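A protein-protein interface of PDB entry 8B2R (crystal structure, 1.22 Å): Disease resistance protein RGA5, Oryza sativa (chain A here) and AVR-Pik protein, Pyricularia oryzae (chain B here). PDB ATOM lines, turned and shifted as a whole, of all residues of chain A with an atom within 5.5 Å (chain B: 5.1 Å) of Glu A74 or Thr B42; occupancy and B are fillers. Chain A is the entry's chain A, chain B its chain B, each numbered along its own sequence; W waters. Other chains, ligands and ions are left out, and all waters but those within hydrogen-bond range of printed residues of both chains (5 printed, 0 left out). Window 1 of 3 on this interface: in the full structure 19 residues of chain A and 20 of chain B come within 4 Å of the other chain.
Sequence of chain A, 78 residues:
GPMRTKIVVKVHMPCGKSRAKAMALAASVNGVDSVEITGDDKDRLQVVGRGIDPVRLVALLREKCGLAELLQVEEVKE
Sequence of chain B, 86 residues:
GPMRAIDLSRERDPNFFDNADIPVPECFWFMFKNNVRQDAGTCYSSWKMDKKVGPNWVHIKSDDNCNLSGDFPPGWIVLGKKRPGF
The backbone NH (N) of Trp B29 is in hydrogen-bond range of the backbone carbonyl oxygen (O) of Gly B41 (2.9 Å). O of Cys B43 is in hydrogen-bond range of N of Cys B27, at 2.9 Å. The indole nitrogen (NE1) of Trp B29 sits at hydrogen-bond distance from the backbone carbonyl oxygen (O) of Thr B42. The backbone NH (N) of Lys A6 sits at hydrogen-bond distance from the backbone carbonyl oxygen (O) of Glu A74 (2.8 Å). The side-chain amide nitrogen (NE2) of Gln A72 lies within hydrogen-bond range of the side-chain carboxylate (OE1) of Glu A74 (3.0 Å). The backbone NH (N) of Val A76 lies within hydrogen-bond range of the backbone carbonyl oxygen (O) of Arg A4, at 2.8 Å.
Glu A74 touches just these residues of chain B: Thr B42, Cys B43, Tyr B44, Trp B47, Lys B48 and Met B49. Printed residues of chain A within 4 Å of Thr B42: Lys A6 (2.9 Å), Gln A72 (3.0 Å) and Glu A74 (3.9 Å). Of the printed residues of chain B, Val A73 touches Met B49 and Asp B50. Of the printed residues of chain A, Met B49 touches Gln A72 (3.6 Å), Val A73 (3.6 Å) and Glu A74 (3.9 Å). The nearest printed residue of chain B that does not touch Glu A74 is Asp B50 (5.1 Å). The nearest printed residue of chain B that does not touch Gln A72 is Cys B43 (4.3 Å).
NE2 of Gln A72 lies within hydrogen-bond range of O of Thr B42, at 3.0 Å. The indole nitrogen (NE1) of Trp B29 lies within hydrogen-bond range of the side-chain amide oxygen (OE1) of Gln A72 (3.4 Å). The side-chain carboxylate (OE1) of Glu A75 lies within salt-bridge range of the side-chain amino group (NZ) of Lys B48 (2.6 Å). The side-chain amino group (NZ) of Lys A6 sits at hydrogen-bond distance from the side-chain hydroxyl (OG1) of Thr B42 (2.9 Å). The side-chain sulfur (SD) of Met B49 sits at hydrogen-bond distance from the side-chain amide nitrogen (NE2) of Gln A72 (3.6 Å). The backbone NH (N) of Val A73 is in hydrogen-bond range of the backbone carbonyl oxygen (O) of Asp B50. The side-chain carboxylate of Glu A74 sits at hydrogen-bond distance from the backbone NH of Tyr B44, at 2.8 Å. The indole nitrogen (NE1) of Trp B47 is in hydrogen-bond range of the backbone carbonyl oxygen (O) of Glu A75 (2.8 Å).
Water W1 lies within hydrogen-bond range of the backbone carbonyl oxygen of Lys B48 and the backbone NH of Glu A75. Water W5 lies within hydrogen-bond range of OE2 of Glu A74 (2.8 Å), O of Tyr B44 (2.8 Å) and N of Lys B48 (3.2 Å). Water W4 bridges the side-chain amino group (NZ) of Lys A6 (2.8 Å) and the side-chain hydroxyl (OG1) of Thr B42 (3.5 Å). Water W3 lies within hydrogen-bond range of OE1 of Glu A74 (2.8 Å), NZ of Lys A6 (2.9 Å) and O of Thr B42 (3.3 Å). Water W2 lies within hydrogen-bond range of the side-chain amide oxygen of Gln A72 (2.8 Å), the side-chain amino group of Lys A6 (2.9 Å) and the backbone NH of Thr B42 (3.0 Å).
Hydrophobic or aromatic side chains of chain B within 4 Å of the printed part of chain A: Trp B29, Tyr B44, Trp B47 and Met B49. Hydrophobic or aromatic side chains of chain A that line the printed part of chain B: Val A76. Among the printed residues, 17 pairs touch across the chains.
Among the printed residues, merely in contact across the chains: Gln A72 with Asp B50, Val A73 with Met B49, Glu A74 with Thr B42, Glu A74 with Cys B43, Glu A74 with Trp B47, Glu A74 with Lys B48, Glu A74 with Met B49, Glu A75 with Tyr B44 and Val A76 with Tyr B44.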
ATOM      1  N   ARG A   4      -9.870   4.199  -7.356  1.00  0.00           N
ATOM      2  CA  ARG A   4     -10.834   3.112  -7.557  1.00  0.00           C
ATOM      3  C   ARG A   4     -11.598   3.341  -8.857  1.00  0.00           C
ATOM      4  O   ARG A   4     -11.633   4.445  -9.399  1.00  0.00           O
ATOM      5  CB  ARG A   4     -11.836   3.086  -6.406  1.00  0.00           C
ATOM      6  CG  ARG A   4     -11.167   2.792  -5.083  1.00  0.00           C
ATOM      7  CD  ARG A   4     -12.069   2.448  -3.924  1.00  0.00           C
ATOM      8  NE  ARG A   4     -12.738   3.615  -3.451  1.00  0.00           N
ATOM      9  CZ  ARG A   4     -13.746   3.593  -2.593  1.00  0.00           C
ATOM     10  NH1 ARG A   4     -14.235   2.440  -2.139  1.00  0.00           N
ATOM     11  NH2 ARG A   4     -14.210   4.745  -2.160  1.00  0.00           N
ATOM     12  N   THR A   5     -12.193   2.294  -9.408  1.00  0.00           N
ATOM     13  CA  THR A   5     -12.938   2.404 -10.648  1.00  0.00           C
ATOM     14  C   THR A   5     -14.175   1.522 -10.579  1.00  0.00           C
ATOM     15  O   THR A   5     -14.144   0.388 -10.059  1.00  0.00           O
ATOM     16  CB  THR A   5     -12.151   1.956 -11.884  1.00  0.00           C
ATOM     17  OG1 THR A   5     -11.926   0.558 -11.716  1.00  0.00           O
ATOM     18  CG2 THR A   5     -10.851   2.703 -12.083  1.00  0.00           C
ATOM     19  N   LYS A   6     -15.250   2.080 -11.148  1.00  0.00           N
ATOM     20  CA  LYS A   6     -16.553   1.466 -11.373  1.00  0.00           C
ATOM     21  C   LYS A   6     -16.597   0.917 -12.788  1.00  0.00           C
ATOM     22  O   LYS A   6     -16.308   1.657 -13.734  1.00  0.00           O
ATOM     23  CB  LYS A   6     -17.673   2.514 -11.220  1.00  0.00           C
ATOM     24  CG  LYS A   6     -19.052   2.183 -11.815  1.00  0.00           C
ATOM     25  CD  LYS A   6     -20.163   3.310 -11.655  1.00  0.00           C
ATOM     26  CE  LYS A   6     -21.439   3.102 -12.470  1.00  0.00           C
ATOM     27  NZ  LYS A   6     -22.563   4.099 -12.262  1.00  0.00           N
ATOM     28  N   ILE A   7     -16.972  -0.357 -12.914  1.00  0.00           N
ATOM     29  CA  ILE A   7     -17.093  -0.990 -14.213  1.00  0.00           C
ATOM     30  C   ILE A   7     -18.481  -1.607 -14.311  1.00  0.00           C
ATOM     31  O   ILE A   7     -18.895  -2.308 -13.387  1.00  0.00           O
ATOM     32  CB  ILE A   7     -16.014  -2.081 -14.373  1.00  0.00           C
ATOM     33  CG1 ILE A   7     -14.590  -1.570 -14.190  1.00  0.00           C
ATOM     34  CG2 ILE A   7     -16.154  -2.782 -15.723  1.00  0.00           C
ATOM     35  CD1 ILE A   7     -13.597  -2.631 -13.902  1.00  0.00           C
ATOM     36  N   GLN A  72     -19.545   0.580 -19.320  1.00  0.00           N
ATOM     37  CA  GLN A  72     -19.074   1.822 -18.686  1.00  0.00           C
ATOM     38  C   GLN A  72     -17.848   1.528 -17.842  1.00  0.00           C
ATOM     39  O   GLN A  72     -17.835   0.513 -17.107  1.00  0.00           O
ATOM     40  CB  GLN A  72     -20.204   2.392 -17.824  1.00  0.00           C
ATOM     41  CG  GLN A  72     -19.909   3.752 -17.184  1.00  0.00           C
ATOM     42  CD  GLN A  72     -21.120   4.258 -16.403  1.00  0.00           C
ATOM     43  OE1 GLN A  72     -22.252   3.851 -16.651  1.00  0.00           O
ATOM     44  NE2 GLN A  72     -20.883   5.185 -15.471  1.00  0.00           N
ATOM     45  N   VAL A  73     -16.830   2.360 -17.980  1.00  0.00           N
ATOM     46  CA  VAL A  73     -15.699   2.371 -17.075  1.00  0.00           C
ATOM     47  C   VAL A  73     -15.563   3.799 -16.577  1.00  0.00           C
ATOM     48  O   VAL A  73     -15.437   4.720 -17.366  1.00  0.00           O
ATOM     49  CB  VAL A  73     -14.394   1.864 -17.726  1.00  0.00           C
ATOM     50  CG1 VAL A  73     -13.245   1.912 -16.711  1.00  0.00           C
ATOM     51  CG2 VAL A  73     -14.539   0.471 -18.278  1.00  0.00           C
ATOM     52  N   GLU A  74     -15.574   4.006 -15.256  1.00  0.00           N
ATOM     53  CA  GLU A  74     -15.539   5.335 -14.674  1.00  0.00           C
ATOM     54  C   GLU A  74     -14.682   5.271 -13.427  1.00  0.00           C
ATOM     55  O   GLU A  74     -14.983   4.545 -12.485  1.00  0.00           O
ATOM     56  CB  GLU A  74     -16.951   5.814 -14.371  1.00  0.00           C
ATOM     57  CG  GLU A  74     -16.997   7.244 -13.924  1.00  0.00           C
ATOM     58  CD  GLU A  74     -18.384   7.804 -13.705  1.00  0.00           C
ATOM     59  OE1 GLU A  74     -19.365   6.989 -13.652  1.00  0.00           O
ATOM     60  OE2 GLU A  74     -18.513   9.031 -13.629  1.00  0.00           O
ATOM     61  N   GLU A  75     -13.613   6.101 -13.386  1.00  0.00           N
ATOM     62  CA  GLU A  75     -12.865   6.255 -12.158  1.00  0.00           C
ATOM     63  C   GLU A  75     -13.825   6.775 -11.099  1.00  0.00           C
ATOM     64  O   GLU A  75     -14.660   7.615 -11.376  1.00  0.00           O
ATOM     65  CB  GLU A  75     -11.715   7.218 -12.385  1.00  0.00           C
ATOM     66  CG  GLU A  75     -10.553   6.628 -13.209  1.00  0.00           C
ATOM     67  CD  GLU A  75      -9.342   7.514 -13.371  1.00  0.00           C
ATOM     68  OE1 GLU A  75      -9.515   8.749 -13.216  1.00  0.00           O
ATOM     69  OE2 GLU A  75      -8.251   6.941 -13.594  1.00  0.00           O
ATOM     70  N   VAL A  76     -13.620   6.379  -9.837  1.00  0.00           N
ATOM     71  CA  VAL A  76     -14.390   6.908  -8.739  1.00  0.00           C
ATOM     72  C   VAL A  76     -13.808   8.269  -8.384  1.00  0.00           C
ATOM     73  O   VAL A  76     -12.633   8.374  -8.044  1.00  0.00           O
ATOM     74  CB  VAL A  76     -14.391   5.967  -7.548  1.00  0.00           C
ATOM     75  CG1 VAL A  76     -15.129   6.586  -6.375  1.00  0.00           C
ATOM     76  CG2 VAL A  76     -14.989   4.598  -7.905  1.00  0.00           C
ATOM     77  N   PHE B  16     -30.738   1.858 -11.402  1.00  0.00           N
ATOM     78  CA  PHE B  16     -29.374   1.960 -10.887  1.00  0.00           C
ATOM     79  C   PHE B  16     -29.343   1.644  -9.398  1.00  0.00           C
ATOM     80  O   PHE B  16     -30.384   1.557  -8.712  1.00  0.00           O
ATOM     81  CB  PHE B  16     -28.811   3.355 -11.167  1.00  0.00           C
ATOM     82  CG  PHE B  16     -29.489   4.375 -10.302  1.00  0.00           C
ATOM     83  CD1 PHE B  16     -30.785   4.804 -10.608  1.00  0.00           C
ATOM     84  CD2 PHE B  16     -28.861   4.869  -9.182  1.00  0.00           C
ATOM     85  CE1 PHE B  16     -31.445   5.693  -9.780  1.00  0.00           C
ATOM     86  CE2 PHE B  16     -29.552   5.709  -8.341  1.00  0.00           C
ATOM     87  CZ  PHE B  16     -30.822   6.122  -8.627  1.00  0.00           C
ATOM     88  N   ASP B  18     -26.826   2.949  -6.082  1.00  0.00           N
ATOM     89  CA  ASP B  18     -25.728   3.745  -5.536  1.00  0.00           C
ATOM     90  C   ASP B  18     -24.924   2.867  -4.539  1.00  0.00           C
ATOM     91  O   ASP B  18     -25.345   2.608  -3.435  1.00  0.00           O
ATOM     92  CB  ASP B  18     -26.257   4.989  -4.821  1.00  0.00           C
ATOM     93  CG  ASP B  18     -26.920   5.996  -5.756  1.00  0.00           C
ATOM     94  OD1 ASP B  18     -26.361   6.248  -6.850  1.00  0.00           O
ATOM     95  OD2 ASP B  18     -27.962   6.567  -5.346  1.00  0.00           O
ATOM     96  N   PRO B  25     -22.854   9.393  -7.264  1.00  0.00           N
ATOM     97  CA  PRO B  25     -22.681  10.165  -8.474  1.00  0.00           C
ATOM     98  C   PRO B  25     -23.797  11.194  -8.675  1.00  0.00           C
ATOM     99  O   PRO B  25     -24.935  10.904  -8.394  1.00  0.00           O
ATOM    100  CB  PRO B  25     -22.585   9.135  -9.589  1.00  0.00           C
ATOM    101  CG  PRO B  25     -23.414   7.980  -9.037  1.00  0.00           C
ATOM    102  CD  PRO B  25     -23.091   7.974  -7.544  1.00  0.00           C
ATOM    103  N   CYS B  27     -24.923  12.714 -11.464  1.00  0.00           N
ATOM    104  CA  CYS B  27     -25.627  12.832 -12.718  1.00  0.00           C
ATOM    105  C   CYS B  27     -26.375  11.543 -13.034  1.00  0.00           C
ATOM    106  O   CYS B  27     -25.908  10.426 -12.780  1.00  0.00           O
ATOM    107  CB  CYS B  27     -24.702  13.123 -13.915  1.00  0.00           C
ATOM    108  SG  CYS B  27     -23.487  14.442 -13.661  1.00  0.00           S
ATOM    109  N   PHE B  28     -27.484  11.734 -13.735  1.00  0.00           N
ATOM    110  CA  PHE B  28     -28.083  10.688 -14.547  1.00  0.00           C
ATOM    111  C   PHE B  28     -27.671  10.926 -15.996  1.00  0.00           C
ATOM    112  O   PHE B  28     -27.592  12.074 -16.453  1.00  0.00           O
ATOM    113  CB  PHE B  28     -29.610  10.660 -14.515  1.00  0.00           C
ATOM    114  CG  PHE B  28     -30.239  10.256 -13.209  1.00  0.00           C
ATOM    115  CD1 PHE B  28     -29.665   9.256 -12.420  1.00  0.00           C
ATOM    116  CD2 PHE B  28     -31.396  10.848 -12.749  1.00  0.00           C
ATOM    117  CE1 PHE B  28     -30.281   8.796 -11.269  1.00  0.00           C
ATOM    118  CE2 PHE B  28     -32.015  10.375 -11.596  1.00  0.00           C
ATOM    119  CZ  PHE B  28     -31.422   9.398 -10.827  1.00  0.00           C
ATOM    120  N   TRP B  29     -27.344   9.852 -16.708  1.00  0.00           N
ATOM    121  CA  TRP B  29     -27.159   9.903 -18.131  1.00  0.00           C
ATOM    122  C   TRP B  29     -28.214   9.032 -18.793  1.00  0.00           C
ATOM    123  O   TRP B  29     -28.697   8.030 -18.237  1.00  0.00           O
ATOM    124  CB  TRP B  29     -25.725   9.513 -18.585  1.00  0.00           C
ATOM    125  CG  TRP B  29     -25.326   8.124 -18.218  1.00  0.00           C
ATOM    126  CD1 TRP B  29     -24.541   7.802 -17.145  1.00  0.00           C
ATOM    127  CD2 TRP B  29     -25.682   6.894 -18.866  1.00  0.00           C
ATOM    128  NE1 TRP B  29     -24.419   6.462 -17.095  1.00  0.00           N
ATOM    129  CE2 TRP B  29     -25.080   5.864 -18.124  1.00  0.00           C
ATOM    130  CE3 TRP B  29     -26.411   6.590 -20.036  1.00  0.00           C
ATOM    131  CZ2 TRP B  29     -25.249   4.519 -18.438  1.00  0.00           C
ATOM    132  CZ3 TRP B  29     -26.535   5.251 -20.352  1.00  0.00           C
ATOM    133  CH2 TRP B  29     -25.978   4.228 -19.562  1.00  0.00           C
ATOM    134  N   ALA B  40     -29.711   3.874 -19.569  1.00  0.00           N
ATOM    135  CA  ALA B  40     -29.591   5.025 -18.685  1.00  0.00           C
ATOM    136  C   ALA B  40     -28.815   4.587 -17.452  1.00  0.00           C
ATOM    137  O   ALA B  40     -28.839   3.403 -17.127  1.00  0.00           O
ATOM    138  CB  ALA B  40     -30.931   5.610 -18.329  1.00  0.00           C
ATOM    139  N   GLY B  41     -28.169   5.518 -16.787  1.00  0.00           N
ATOM    140  CA  GLY B  41     -27.397   5.176 -15.615  1.00  0.00           C
ATOM    141  C   GLY B  41     -26.917   6.406 -14.905  1.00  0.00           C
ATOM    142  O   GLY B  41     -27.507   7.467 -15.025  1.00  0.00           O
ATOM    143  N   THR B  42     -25.830   6.257 -14.134  1.00  0.00           N
ATOM    144  CA  THR B  42     -25.285   7.364 -13.373  1.00  0.00           C
ATOM    145  C   THR B  42     -23.833   7.580 -13.769  1.00  0.00           C
ATOM    146  O   THR B  42     -23.155   6.686 -14.274  1.00  0.00           O
ATOM    147  CB  THR B  42     -25.372   7.113 -11.857  1.00  0.00           C
ATOM    148  OG1 THR B  42     -24.626   5.934 -11.518  1.00  0.00           O
ATOM    149  CG2 THR B  42     -26.802   6.930 -11.397  1.00  0.00           C
ATOM    150  N   CYS B  43     -23.394   8.823 -13.536  1.00  0.00           N
ATOM    151  CA  CYS B  43     -21.997   9.205 -13.679  1.00  0.00           C
ATOM    152  C   CYS B  43     -21.724  10.435 -12.798  1.00  0.00           C
ATOM    153  O   CYS B  43     -22.647  11.125 -12.373  1.00  0.00           O
ATOM    154  CB  CYS B  43     -21.587   9.460 -15.123  1.00  0.00           C
ATOM    155  SG  CYS B  43     -22.402  10.846 -15.922  1.00  0.00           S
ATOM    156  N   TYR B  44     -20.446  10.679 -12.519  1.00  0.00           N
ATOM    157  CA  TYR B  44     -20.056  11.853 -11.715  1.00  0.00           C
ATOM    158  C   TYR B  44     -20.098  13.133 -12.561  1.00  0.00           C
ATOM    159  O   TYR B  44     -19.740  13.062 -13.742  1.00  0.00           O
ATOM    160  CB  TYR B  44     -18.638  11.650 -11.113  1.00  0.00           C
ATOM    161  CG  TYR B  44     -18.612  10.573 -10.069  1.00  0.00           C
ATOM    162  CD1 TYR B  44     -19.138  10.799  -8.809  1.00  0.00           C
ATOM    163  CD2 TYR B  44     -18.075   9.326 -10.322  1.00  0.00           C
ATOM    164  CE1 TYR B  44     -19.160   9.793  -7.844  1.00  0.00           C
ATOM    165  CE2 TYR B  44     -18.089   8.307  -9.361  1.00  0.00           C
ATOM    166  CZ  TYR B  44     -18.671   8.539  -8.149  1.00  0.00           C
ATOM    167  OH  TYR B  44     -18.717   7.504  -7.241  1.00  0.00           O
ATOM    168  N   TRP B  47     -16.288  15.501 -14.388  1.00  0.00           N
ATOM    169  CA  TRP B  47     -15.568  14.242 -14.401  1.00  0.00           C
ATOM    170  C   TRP B  47     -15.546  13.702 -15.837  1.00  0.00           C
ATOM    171  O   TRP B  47     -15.632  14.436 -16.834  1.00  0.00           O
ATOM    172  CB  TRP B  47     -16.127  13.273 -13.338  1.00  0.00           C
ATOM    173  CG  TRP B  47     -15.177  12.215 -12.852  1.00  0.00           C
ATOM    174  CD1 TRP B  47     -15.435  10.862 -12.925  1.00  0.00           C
ATOM    175  CD2 TRP B  47     -13.899  12.384 -12.218  1.00  0.00           C
ATOM    176  NE1 TRP B  47     -14.394  10.187 -12.380  1.00  0.00           N
ATOM    177  CE2 TRP B  47     -13.429  11.079 -11.951  1.00  0.00           C
ATOM    178  CE3 TRP B  47     -13.081  13.482 -11.934  1.00  0.00           C
ATOM    179  CZ2 TRP B  47     -12.189  10.829 -11.347  1.00  0.00           C
ATOM    180  CZ3 TRP B  47     -11.876  13.235 -11.330  1.00  0.00           C
ATOM    181  CH2 TRP B  47     -11.441  11.949 -11.042  1.00  0.00           C
ATOM    182  N   LYS B  48     -15.548  12.363 -15.964  1.00  0.00           N
ATOM    183  CA  LYS B  48     -15.382  11.714 -17.247  1.00  0.00           C
ATOM    184  C   LYS B  48     -15.721  10.254 -17.052  1.00  0.00           C
ATOM    185  O   LYS B  48     -15.525   9.734 -15.955  1.00  0.00           O
ATOM    186  CB  LYS B  48     -13.979  11.902 -17.852  1.00  0.00           C
ATOM    187  CG  LYS B  48     -12.826  11.265 -17.084  1.00  0.00           C
ATOM    188  CD  LYS B  48     -12.599  11.756 -15.647  1.00  0.00           C
ATOM    189  CE  LYS B  48     -11.285  11.326 -15.021  1.00  0.00           C
ATOM    190  NZ  LYS B  48     -11.174   9.857 -14.954  1.00  0.00           N
ATOM    191  N   MET B  49     -16.050   9.584 -18.154  1.00  0.00           N
ATOM    192  CA  MET B  49     -16.243   8.150 -18.194  1.00  0.00           C
ATOM    193  C   MET B  49     -15.973   7.666 -19.613  1.00  0.00           C
ATOM    194  O   MET B  49     -15.974   8.432 -20.561  1.00  0.00           O
ATOM    195  CB  MET B  49     -17.662   7.720 -17.783  1.00  0.00           C
ATOM    196  CG  MET B  49     -18.741   8.186 -18.670  1.00  0.00           C
ATOM    197  SD  MET B  49     -20.346   7.565 -18.181  1.00  0.00           S
ATOM    198  CE  MET B  49     -21.430   8.608 -19.129  1.00  0.00           C
ATOM    199  N   ASP B  50     -15.742   6.369 -19.724  1.00  0.00           N
ATOM    200  CA  ASP B  50     -15.689   5.685 -21.005  1.00  0.00           C
ATOM    201  C   ASP B  50     -16.948   4.839 -21.115  1.00  0.00           C
ATOM    202  O   ASP B  50     -17.311   4.158 -20.158  1.00  0.00           O
ATOM    203  CB  ASP B  50     -14.400   4.899 -21.105  1.00  0.00           C
ATOM    204  CG  ASP B  50     -13.210   5.858 -21.037  1.00  0.00           C
ATOM    205  OD1 ASP B  50     -13.095   6.697 -21.928  1.00  0.00           O
ATOM    206  OD2 ASP B  50     -12.354   5.755 -20.076  1.00  0.00           O
ATOM    207  N   ARG B  83     -28.945  15.028 -10.744  1.00  0.00           N
ATOM    208  CA  ARG B  83     -29.924  14.365  -9.893  1.00  0.00           C
ATOM    209  C   ARG B  83     -30.446  15.303  -8.805  1.00  0.00           C
ATOM    210  O   ARG B  83     -29.749  16.223  -8.366  1.00  0.00           O
ATOM    211  CB  ARG B  83     -29.241  13.176  -9.224  1.00  0.00           C
ATOM    212  CG  ARG B  83     -28.848  12.071 -10.173  1.00  0.00           C
ATOM    213  CD  ARG B  83     -27.983  11.013  -9.515  1.00  0.00           C
ATOM    214  NE  ARG B  83     -28.709  10.324  -8.447  1.00  0.00           N
ATOM    215  CZ  ARG B  83     -28.211   9.282  -7.798  1.00  0.00           C
ATOM    216  NH1 ARG B  83     -26.997   8.815  -8.056  1.00  0.00           N
ATOM    217  NH2 ARG B  83     -28.970   8.657  -6.938  1.00  0.00           N
HETATM  218  O   HOH W   1     -13.414   8.115 -15.401  1.00  0.00           O
HETATM  219  O   HOH W   2     -24.237   3.705 -14.630  1.00  0.00           O
HETATM  220  O   HOH W   3     -21.234   6.597 -11.596  1.00  0.00           O
HETATM  221  O   HOH W   4     -23.676   2.943 -10.003  1.00  0.00           O
HETATM  222  O   HOH W   5     -18.470  11.141 -15.393  1.00  0.00           O
